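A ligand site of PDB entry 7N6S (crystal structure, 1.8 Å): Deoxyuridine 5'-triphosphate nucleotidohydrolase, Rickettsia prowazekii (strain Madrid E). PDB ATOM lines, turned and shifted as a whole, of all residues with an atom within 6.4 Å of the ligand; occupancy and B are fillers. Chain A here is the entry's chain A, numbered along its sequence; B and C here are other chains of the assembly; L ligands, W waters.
The side-chain carboxylate of Asp 91 is in salt-bridge range of the guanidinium group of Arg 142 of chain C, at 3.3 Å.
OG of Ser 73 of chain B is in hydrogen-bond range of ND2 of Asn 85, at 2.9 Å.
The side-chain hydroxyl of Tyr 94 is in hydrogen-bond range of the backbone carbonyl oxygen of Glu 97 (2.7 Å).
The side-chain amide nitrogen of Gln 120 of chain B lies within hydrogen-bond range of the backbone carbonyl oxygen of Pro 71 of chain B.
N of Ile 69 sits at hydrogen-bond distance from O of Gly 88.
The guanidinium group of Arg 142 of chain C lies within salt-bridge range of the side-chain carboxylate of Asp 93, 3.1 Å away.
The guanidinium group (NH1) of Arg 72 of chain B is in salt-bridge range of the side-chain carboxylate (OD1) of Asp 34 of chain B.
Residues that only touch the ligand: Ile 69 (3.7 Å), Gly 88 (3.6 Å), Thr 89 (3.3 Å), Ile 90 (3.4 Å), Tyr 94 (3.4 Å), Glu 97 (3.7 Å), Ile 98 (3.6 Å), Arg 72 of chain B (3.9 Å) and Gln 120 of chain B (3.5 Å).
Hydrophobic or aromatic side chains within 4 Å of the ligand: Ile 69, Ile 90 and Tyr 94.
Of the 25 residues printed, 14 come within 4 Å of the ligand.
N of Asp 91 is in hydrogen-bond range of O3 of the ligand (3.2 Å).
The side-chain carboxylate (OD2) of Asp 91 is in hydrogen-bond range of an oxygen (O3) of the ligand (2.5 Å).
The backbone NH of Ser 73 of chain B lies within hydrogen-bond range of an oxygen (O7) of the ligand, 2.9 Å away.
O7 of the ligand sits at hydrogen-bond distance from OG of Ser 73 of chain B.
The backbone NH of Lys 99 lies within hydrogen-bond range of an oxygen (O1) of the ligand.
A nitrogen (N2) of the ligand sits at hydrogen-bond distance from the backbone carbonyl oxygen (O) of Lys 99, 2.8 Å away.
ND2 of Asn 85 lies within hydrogen-bond range of O2 of the ligand (3.0 Å).
NH2 of Arg 142 of chain C lies within salt-bridge range of O6 of the ligand (3.99 Å).
Water W3 lies within hydrogen-bond range of an oxygen (O7) of the ligand (2.6 Å), the backbone NH (N) of Thr 89 (2.9 Å), the side-chain hydroxyl (OG) of Ser 73 of chain B (3.1 Å) and the side-chain amide nitrogen (NE2) of Gln 120 of chain B (3.4 Å).
Water W1 lies within hydrogen-bond range of O8 of the ligand (2.6 Å), N of Gly 74 of chain B (2.7 Å) and N of Ser 73 of chain B (3.4 Å).
Water W4 lies within hydrogen-bond range of an oxygen (O2) of the ligand, the backbone NH of Leu 101 and the side-chain amide oxygen of Asn 85.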
ATOM      1  N   LEU A  52     -21.798 -27.215 -24.254  1.00  0.00           N
ATOM      2  CA  LEU A  52     -21.289 -25.987 -23.683  1.00  0.00           C
ATOM      3  C   LEU A  52     -20.617 -26.255 -22.342  1.00  0.00           C
ATOM      4  O   LEU A  52     -21.221 -26.886 -21.464  1.00  0.00           O
ATOM      5  CB  LEU A  52     -22.450 -25.005 -23.507  1.00  0.00           C
ATOM      6  CG  LEU A  52     -22.185 -23.526 -23.273  1.00  0.00           C
ATOM      7  CD1 LEU A  52     -21.454 -22.932 -24.462  1.00  0.00           C
ATOM      8  CD2 LEU A  52     -23.531 -22.857 -23.081  1.00  0.00           C
ATOM      9  N   ILE A  69     -11.894 -17.087 -28.628  1.00  0.00           N
ATOM     10  CA  ILE A  69     -11.899 -18.453 -28.095  1.00  0.00           C
ATOM     11  C   ILE A  69     -11.508 -19.401 -29.231  1.00  0.00           C
ATOM     12  O   ILE A  69     -12.260 -19.593 -30.173  1.00  0.00           O
ATOM     13  CB  ILE A  69     -13.271 -18.844 -27.511  1.00  0.00           C
ATOM     14  CG1 ILE A  69     -13.788 -17.799 -26.527  1.00  0.00           C
ATOM     15  CG2 ILE A  69     -13.188 -20.228 -26.860  1.00  0.00           C
ATOM     16  CD1 ILE A  69     -12.846 -17.428 -25.387  1.00  0.00           C
ATOM     17  N   VAL A  83     -13.617 -26.534 -31.141  1.00  0.00           N
ATOM     18  CA  VAL A  83     -14.535 -25.477 -30.719  1.00  0.00           C
ATOM     19  C   VAL A  83     -15.541 -25.228 -31.844  1.00  0.00           C
ATOM     20  O   VAL A  83     -15.165 -24.846 -32.941  1.00  0.00           O
ATOM     21  CB  VAL A  83     -13.746 -24.203 -30.360  1.00  0.00           C
ATOM     22  CG1 VAL A  83     -14.699 -23.016 -30.125  1.00  0.00           C
ATOM     23  CG2 VAL A  83     -12.807 -24.479 -29.129  1.00  0.00           C
ATOM     24  N   ASN A  85     -17.939 -23.086 -32.456  1.00  0.00           N
ATOM     25  CA  ASN A  85     -18.162 -21.738 -32.975  1.00  0.00           C
ATOM     26  C   ASN A  85     -16.848 -20.989 -33.173  1.00  0.00           C
ATOM     27  O   ASN A  85     -16.808 -19.764 -33.078  1.00  0.00           O
ATOM     28  CB  ASN A  85     -19.060 -20.958 -32.031  1.00  0.00           C
ATOM     29  CG  ASN A  85     -18.404 -20.728 -30.697  1.00  0.00           C
ATOM     30  OD1 ASN A  85     -17.587 -21.542 -30.281  1.00  0.00           O
ATOM     31  ND2 ASN A  85     -18.721 -19.624 -30.042  1.00  0.00           N
ATOM     32  N   PRO A  87     -13.552 -19.009 -34.458  1.00  0.00           N
ATOM     33  CA  PRO A  87     -13.118 -18.526 -33.157  1.00  0.00           C
ATOM     34  C   PRO A  87     -14.294 -17.819 -32.482  1.00  0.00           C
ATOM     35  O   PRO A  87     -14.969 -17.030 -33.138  1.00  0.00           O
ATOM     36  CB  PRO A  87     -11.986 -17.552 -33.496  1.00  0.00           C
ATOM     37  CG  PRO A  87     -12.329 -17.066 -34.880  1.00  0.00           C
ATOM     38  CD  PRO A  87     -13.073 -18.155 -35.563  1.00  0.00           C
ATOM     39  N   GLY A  88     -14.537 -18.167 -31.215  1.00  0.00           N
ATOM     40  CA  GLY A  88     -15.590 -17.503 -30.460  1.00  0.00           C
ATOM     41  C   GLY A  88     -15.185 -16.080 -30.163  1.00  0.00           C
ATOM     42  O   GLY A  88     -14.023 -15.790 -29.867  1.00  0.00           O
ATOM     43  N   THR A  89     -16.138 -15.159 -30.291  1.00  0.00           N
ATOM     44  CA  THR A  89     -15.853 -13.730 -30.124  1.00  0.00           C
ATOM     45  C   THR A  89     -16.374 -13.263 -28.772  1.00  0.00           C
ATOM     46  O   THR A  89     -17.586 -13.316 -28.528  1.00  0.00           O
ATOM     47  CB  THR A  89     -16.518 -12.937 -31.250  1.00  0.00           C
ATOM     48  OG1 THR A  89     -15.937 -13.326 -32.510  1.00  0.00           O
ATOM     49  CG2 THR A  89     -16.294 -11.451 -31.059  1.00  0.00           C
ATOM     50  N   ILE A  90     -15.474 -12.781 -27.899  1.00  0.00           N
ATOM     51  CA  ILE A  90     -15.869 -12.206 -26.611  1.00  0.00           C
ATOM     52  C   ILE A  90     -15.841 -10.692 -26.766  1.00  0.00           C
ATOM     53  O   ILE A  90     -14.773 -10.109 -26.987  1.00  0.00           O
ATOM     54  CB  ILE A  90     -14.946 -12.631 -25.457  1.00  0.00           C
ATOM     55  CG1 ILE A  90     -14.728 -14.164 -25.414  1.00  0.00           C
ATOM     56  CG2 ILE A  90     -15.494 -12.056 -24.151  1.00  0.00           C
ATOM     57  CD1 ILE A  90     -15.979 -15.030 -25.348  1.00  0.00           C
ATOM     58  N   ASP A  91     -17.008 -10.065 -26.680  1.00  0.00           N
ATOM     59  CA  ASP A  91     -17.133  -8.624 -26.844  1.00  0.00           C
ATOM     60  C   ASP A  91     -16.732  -7.855 -25.584  1.00  0.00           C
ATOM     61  O   ASP A  91     -16.878  -8.345 -24.466  1.00  0.00           O
ATOM     62  CB  ASP A  91     -18.574  -8.293 -27.230  1.00  0.00           C
ATOM     63  CG  ASP A  91     -18.990  -9.000 -28.513  1.00  0.00           C
ATOM     64  OD1 ASP A  91     -18.503  -8.602 -29.583  1.00  0.00           O
ATOM     65  OD2 ASP A  91     -19.704 -10.017 -28.433  1.00  0.00           O
ATOM     66  N   ALA A  92     -16.257  -6.621 -25.788  1.00  0.00           N
ATOM     67  CA  ALA A  92     -15.809  -5.809 -24.677  1.00  0.00           C
ATOM     68  C   ALA A  92     -16.934  -5.482 -23.706  1.00  0.00           C
ATOM     69  O   ALA A  92     -16.670  -5.195 -22.542  1.00  0.00           O
ATOM     70  CB  ALA A  92     -15.166  -4.505 -25.182  1.00  0.00           C
ATOM     71  N   ASP A  93     -18.202  -5.528 -24.138  1.00  0.00           N
ATOM     72  CA  ASP A  93     -19.287  -5.268 -23.192  1.00  0.00           C
ATOM     73  C   ASP A  93     -19.984  -6.544 -22.692  1.00  0.00           C
ATOM     74  O   ASP A  93     -21.033  -6.441 -22.040  1.00  0.00           O
ATOM     75  CB  ASP A  93     -20.307  -4.298 -23.798  1.00  0.00           C
ATOM     76  CG  ASP A  93     -20.830  -4.738 -25.147  1.00  0.00           C
ATOM     77  OD1 ASP A  93     -20.490  -5.839 -25.630  1.00  0.00           O
ATOM     78  OD2 ASP A  93     -21.608  -3.961 -25.729  1.00  0.00           O
ATOM     79  N   TYR A  94     -19.428  -7.710 -22.937  1.00  0.00           N
ATOM     80  CA  TYR A  94     -20.013  -8.932 -22.400  1.00  0.00           C
ATOM     81  C   TYR A  94     -19.677  -9.029 -20.928  1.00  0.00           C
ATOM     82  O   TYR A  94     -18.517  -8.865 -20.537  1.00  0.00           O
ATOM     83  CB  TYR A  94     -19.501 -10.154 -23.138  1.00  0.00           C
ATOM     84  CG  TYR A  94     -20.042 -11.471 -22.625  1.00  0.00           C
ATOM     85  CD1 TYR A  94     -21.375 -11.786 -22.783  1.00  0.00           C
ATOM     86  CD2 TYR A  94     -19.220 -12.406 -22.034  1.00  0.00           C
ATOM     87  CE1 TYR A  94     -21.882 -13.001 -22.351  1.00  0.00           C
ATOM     88  CE2 TYR A  94     -19.719 -13.627 -21.602  1.00  0.00           C
ATOM     89  CZ  TYR A  94     -21.055 -13.915 -21.771  1.00  0.00           C
ATOM     90  OH  TYR A  94     -21.594 -15.106 -21.352  1.00  0.00           O
ATOM     91  N   GLY A  96     -21.248 -11.695 -18.964  1.00  0.00           N
ATOM     92  CA  GLY A  96     -21.647 -13.016 -18.531  1.00  0.00           C
ATOM     93  C   GLY A  96     -20.432 -13.909 -18.315  1.00  0.00           C
ATOM     94  O   GLY A  96     -19.290 -13.483 -18.455  1.00  0.00           O
ATOM     95  N   GLU A  97     -20.724 -15.170 -18.017  1.00  0.00           N
ATOM     96  CA  GLU A  97     -19.684 -16.193 -17.889  1.00  0.00           C
ATOM     97  C   GLU A  97     -19.159 -16.587 -19.253  1.00  0.00           C
ATOM     98  O   GLU A  97     -19.932 -16.839 -20.184  1.00  0.00           O
ATOM     99  CB  GLU A  97     -20.235 -17.432 -17.199  1.00  0.00           C
ATOM    100  CG  GLU A  97     -19.159 -18.532 -17.006  1.00  0.00           C
ATOM    101  CD  GLU A  97     -19.678 -19.674 -16.156  1.00  0.00           C
ATOM    102  OE1 GLU A  97     -20.906 -19.692 -15.874  1.00  0.00           O
ATOM    103  OE2 GLU A  97     -18.870 -20.533 -15.730  1.00  0.00           O
ATOM    104  N   ILE A  98     -17.839 -16.642 -19.376  1.00  0.00           N
ATOM    105  CA  ILE A  98     -17.235 -17.162 -20.579  1.00  0.00           C
ATOM    106  C   ILE A  98     -17.465 -18.658 -20.660  1.00  0.00           C
ATOM    107  O   ILE A  98     -17.168 -19.398 -19.713  1.00  0.00           O
ATOM    108  CB  ILE A  98     -15.736 -16.815 -20.611  1.00  0.00           C
ATOM    109  CG1 ILE A  98     -15.550 -15.317 -20.834  1.00  0.00           C
ATOM    110  CG2 ILE A  98     -15.039 -17.618 -21.719  1.00  0.00           C
ATOM    111  CD1 ILE A  98     -14.135 -14.876 -20.704  1.00  0.00           C
ATOM    112  N   LYS A  99     -18.015 -19.107 -21.790  1.00  0.00           N
ATOM    113  CA  LYS A  99     -18.278 -20.514 -22.007  1.00  0.00           C
ATOM    114  C   LYS A  99     -17.607 -20.956 -23.309  1.00  0.00           C
ATOM    115  O   LYS A  99     -17.393 -20.147 -24.221  1.00  0.00           O
ATOM    116  CB  LYS A  99     -19.774 -20.798 -22.047  1.00  0.00           C
ATOM    117  CG  LYS A  99     -20.436 -20.375 -20.724  1.00  0.00           C
ATOM    118  CD  LYS A  99     -21.868 -20.747 -20.667  1.00  0.00           C
ATOM    119  CE  LYS A  99     -22.450 -20.347 -19.317  1.00  0.00           C
ATOM    120  NZ  LYS A  99     -23.922 -20.562 -19.318  1.00  0.00           N
ATOM    121  N   VAL A 100     -17.222 -22.224 -23.352  1.00  0.00           N
ATOM    122  CA  VAL A 100     -16.567 -22.820 -24.509  1.00  0.00           C
ATOM    123  C   VAL A 100     -17.512 -23.848 -25.098  1.00  0.00           C
ATOM    124  O   VAL A 100     -17.940 -24.768 -24.389  1.00  0.00           O
ATOM    125  CB  VAL A 100     -15.233 -23.482 -24.121  1.00  0.00           C
ATOM    126  CG1 VAL A 100     -14.585 -24.196 -25.335  1.00  0.00           C
ATOM    127  CG2 VAL A 100     -14.284 -22.445 -23.502  1.00  0.00           C
ATOM    128  N   LEU A 101     -17.786 -23.727 -26.386  1.00  0.00           N
ATOM    129  CA  LEU A 101     -18.716 -24.615 -27.099  1.00  0.00           C
ATOM    130  C   LEU A 101     -17.885 -25.662 -27.848  1.00  0.00           C
ATOM    131  O   LEU A 101     -17.219 -25.348 -28.843  1.00  0.00           O
ATOM    132  CB  LEU A 101     -19.610 -23.805 -28.042  1.00  0.00           C
ATOM    133  CG  LEU A 101     -20.742 -24.646 -28.620  1.00  0.00           C
ATOM    134  CD1 LEU A 101     -21.788 -24.904 -27.545  1.00  0.00           C
ATOM    135  CD2 LEU A 101     -21.365 -23.944 -29.851  1.00  0.00           C
ATOM    136  N   ASP B  34     -23.206  -7.964 -37.650  1.00  0.00           N
ATOM    137  CA  ASP B  34     -23.956  -9.142 -38.049  1.00  0.00           C
ATOM    138  C   ASP B  34     -24.120  -9.172 -39.565  1.00  0.00           C
ATOM    139  O   ASP B  34     -24.474  -8.147 -40.174  1.00  0.00           O
ATOM    140  CB  ASP B  34     -25.329  -9.186 -37.366  1.00  0.00           C
ATOM    141  CG  ASP B  34     -25.238  -9.238 -35.853  1.00  0.00           C
ATOM    142  OD1 ASP B  34     -24.268  -9.796 -35.304  1.00  0.00           O
ATOM    143  OD2 ASP B  34     -26.161  -8.731 -35.194  1.00  0.00           O
ATOM    144  N   PRO B  71     -18.378 -17.419 -36.715  1.00  0.00           N
ATOM    145  CA  PRO B  71     -19.719 -17.901 -36.377  1.00  0.00           C
ATOM    146  C   PRO B  71     -20.451 -17.022 -35.354  1.00  0.00           C
ATOM    147  O   PRO B  71     -19.842 -16.410 -34.476  1.00  0.00           O
ATOM    148  CB  PRO B  71     -19.462 -19.313 -35.803  1.00  0.00           C
ATOM    149  CG  PRO B  71     -18.046 -19.668 -36.250  1.00  0.00           C
ATOM    150  CD  PRO B  71     -17.314 -18.355 -36.298  1.00  0.00           C
ATOM    151  N   ARG B  72     -21.786 -17.000 -35.472  1.00  0.00           N
ATOM    152  CA  ARG B  72     -22.632 -16.535 -34.385  1.00  0.00           C
ATOM    153  C   ARG B  72     -22.864 -17.680 -33.413  1.00  0.00           C
ATOM    154  O   ARG B  72     -23.215 -18.793 -33.826  1.00  0.00           O
ATOM    155  CB  ARG B  72     -23.992 -16.062 -34.910  1.00  0.00           C
ATOM    156  CG  ARG B  72     -23.941 -15.175 -36.117  1.00  0.00           C
ATOM    157  CD  ARG B  72     -25.359 -14.712 -36.506  1.00  0.00           C
ATOM    158  NE  ARG B  72     -26.052 -14.150 -35.350  1.00  0.00           N
ATOM    159  CZ  ARG B  72     -25.725 -12.986 -34.820  1.00  0.00           C
ATOM    160  NH1 ARG B  72     -24.752 -12.250 -35.344  1.00  0.00           N
ATOM    161  NH2 ARG B  72     -26.379 -12.551 -33.748  1.00  0.00           N
ATOM    162  N   SER B  73     -22.700 -17.409 -32.116  1.00  0.00           N
ATOM    163  CA  SER B  73     -22.806 -18.523 -31.166  1.00  0.00           C
ATOM    164  C   SER B  73     -24.210 -19.090 -31.091  1.00  0.00           C
ATOM    165  O   SER B  73     -24.374 -20.306 -30.865  1.00  0.00           O
ATOM    166  CB  SER B  73     -22.338 -18.068 -29.792  1.00  0.00           C
ATOM    167  OG  SER B  73     -20.952 -17.812 -29.869  1.00  0.00           O
ATOM    168  N   GLY B  74     -25.243 -18.269 -31.292  1.00  0.00           N
ATOM    169  CA  GLY B  74     -26.600 -18.772 -31.215  1.00  0.00           C
ATOM    170  C   GLY B  74     -26.911 -19.875 -32.217  1.00  0.00           C
ATOM    171  O   GLY B  74     -27.522 -20.887 -31.869  1.00  0.00           O
ATOM    172  N   GLN B 120     -20.873 -13.257 -38.109  1.00  0.00           N
ATOM    173  CA  GLN B 120     -20.484 -11.924 -37.690  1.00  0.00           C
ATOM    174  C   GLN B 120     -19.156 -11.586 -38.356  1.00  0.00           C
ATOM    175  O   GLN B 120     -18.396 -12.464 -38.755  1.00  0.00           O
ATOM    176  CB  GLN B 120     -20.411 -11.765 -36.175  1.00  0.00           C
ATOM    177  CG  GLN B 120     -19.500 -12.682 -35.458  1.00  0.00           C
ATOM    178  CD  GLN B 120     -19.551 -12.455 -33.944  1.00  0.00           C
ATOM    179  OE1 GLN B 120     -19.391 -11.339 -33.475  1.00  0.00           O
ATOM    180  NE2 GLN B 120     -19.789 -13.516 -33.177  1.00  0.00           N
ATOM    181  N   ARG C 142     -25.223  -4.556 -23.026  1.00  0.00           N
ATOM    182  CA  ARG C 142     -25.291  -5.967 -23.358  1.00  0.00           C
ATOM    183  C   ARG C 142     -25.660  -6.756 -22.107  1.00  0.00           C
ATOM    184  O   ARG C 142     -26.807  -7.167 -21.937  1.00  0.00           O
ATOM    185  CB  ARG C 142     -23.961  -6.454 -23.928  1.00  0.00           C
ATOM    186  CG  ARG C 142     -23.980  -7.860 -24.468  1.00  0.00           C
ATOM    187  CD  ARG C 142     -22.620  -8.270 -25.018  1.00  0.00           C
ATOM    188  NE  ARG C 142     -22.834  -9.080 -26.203  1.00  0.00           N
ATOM    189  CZ  ARG C 142     -22.615  -8.678 -27.443  1.00  0.00           C
ATOM    190  NH1 ARG C 142     -22.024  -7.529 -27.696  1.00  0.00           N
ATOM    191  NH2 ARG C 142     -22.997  -9.455 -28.450  1.00  0.00           N
HETATM  192  N1  LIG L   1     -19.352 -15.956 -25.767  1.00  0.00           N
HETATM  193  C1  LIG L   1     -18.752 -16.930 -24.981  1.00  0.00           C
HETATM  194  N2  LIG L   1     -18.047 -17.885 -25.662  1.00  0.00           N
HETATM  195  C2  LIG L   1     -17.885 -17.961 -27.032  1.00  0.00           C
HETATM  196  C3  LIG L   1     -18.552 -16.938 -27.785  1.00  0.00           C
HETATM  197  C4  LIG L   1     -19.258 -16.006 -27.143  1.00  0.00           C
HETATM  198  O1  LIG L   1     -18.850 -16.936 -23.754  1.00  0.00           O
HETATM  199  O2  LIG L   1     -17.194 -18.860 -27.526  1.00  0.00           O
HETATM  200  C5  LIG L   1     -20.025 -14.825 -25.098  1.00  0.00           C
HETATM  201  C6  LIG L   1     -19.277 -13.507 -25.285  1.00  0.00           C
HETATM  202  C7  LIG L   1     -20.047 -12.823 -26.416  1.00  0.00           C
HETATM  203  C8  LIG L   1     -21.465 -13.321 -26.183  1.00  0.00           C
HETATM  204  O3  LIG L   1     -19.931 -11.393 -26.311  1.00  0.00           O
HETATM  205  O4  LIG L   1     -21.312 -14.666 -25.699  1.00  0.00           O
HETATM  206  C9  LIG L   1     -22.355 -13.330 -27.401  1.00  0.00           C
HETATM  207  O5  LIG L   1     -21.708 -14.122 -28.423  1.00  0.00           O
HETATM  208  P1  LIG L   1     -22.317 -14.145 -29.941  1.00  0.00           P
HETATM  209  O6  LIG L   1     -22.120 -12.759 -30.511  1.00  0.00           O
HETATM  210  O7  LIG L   1     -21.539 -15.241 -30.663  1.00  0.00           O
HETATM  211  O8  LIG L   1     -23.820 -14.453 -29.821  1.00  0.00           O
HETATM  212  O   HOH W   1     -25.492 -15.576 -31.533  1.00  0.00           O
HETATM  213  O   HOH W   2     -19.692 -11.916 -30.119  1.00  0.00           O
HETATM  214  O   HOH W   3     -18.950 -15.652 -30.732  1.00  0.00           O
HETATM  215  O   HOH W   4     -16.585 -21.551 -27.629  1.00  0.00           O
HETATM  216  O   HOH W   5     -24.381 -11.397 -25.562  1.00  0.00           O
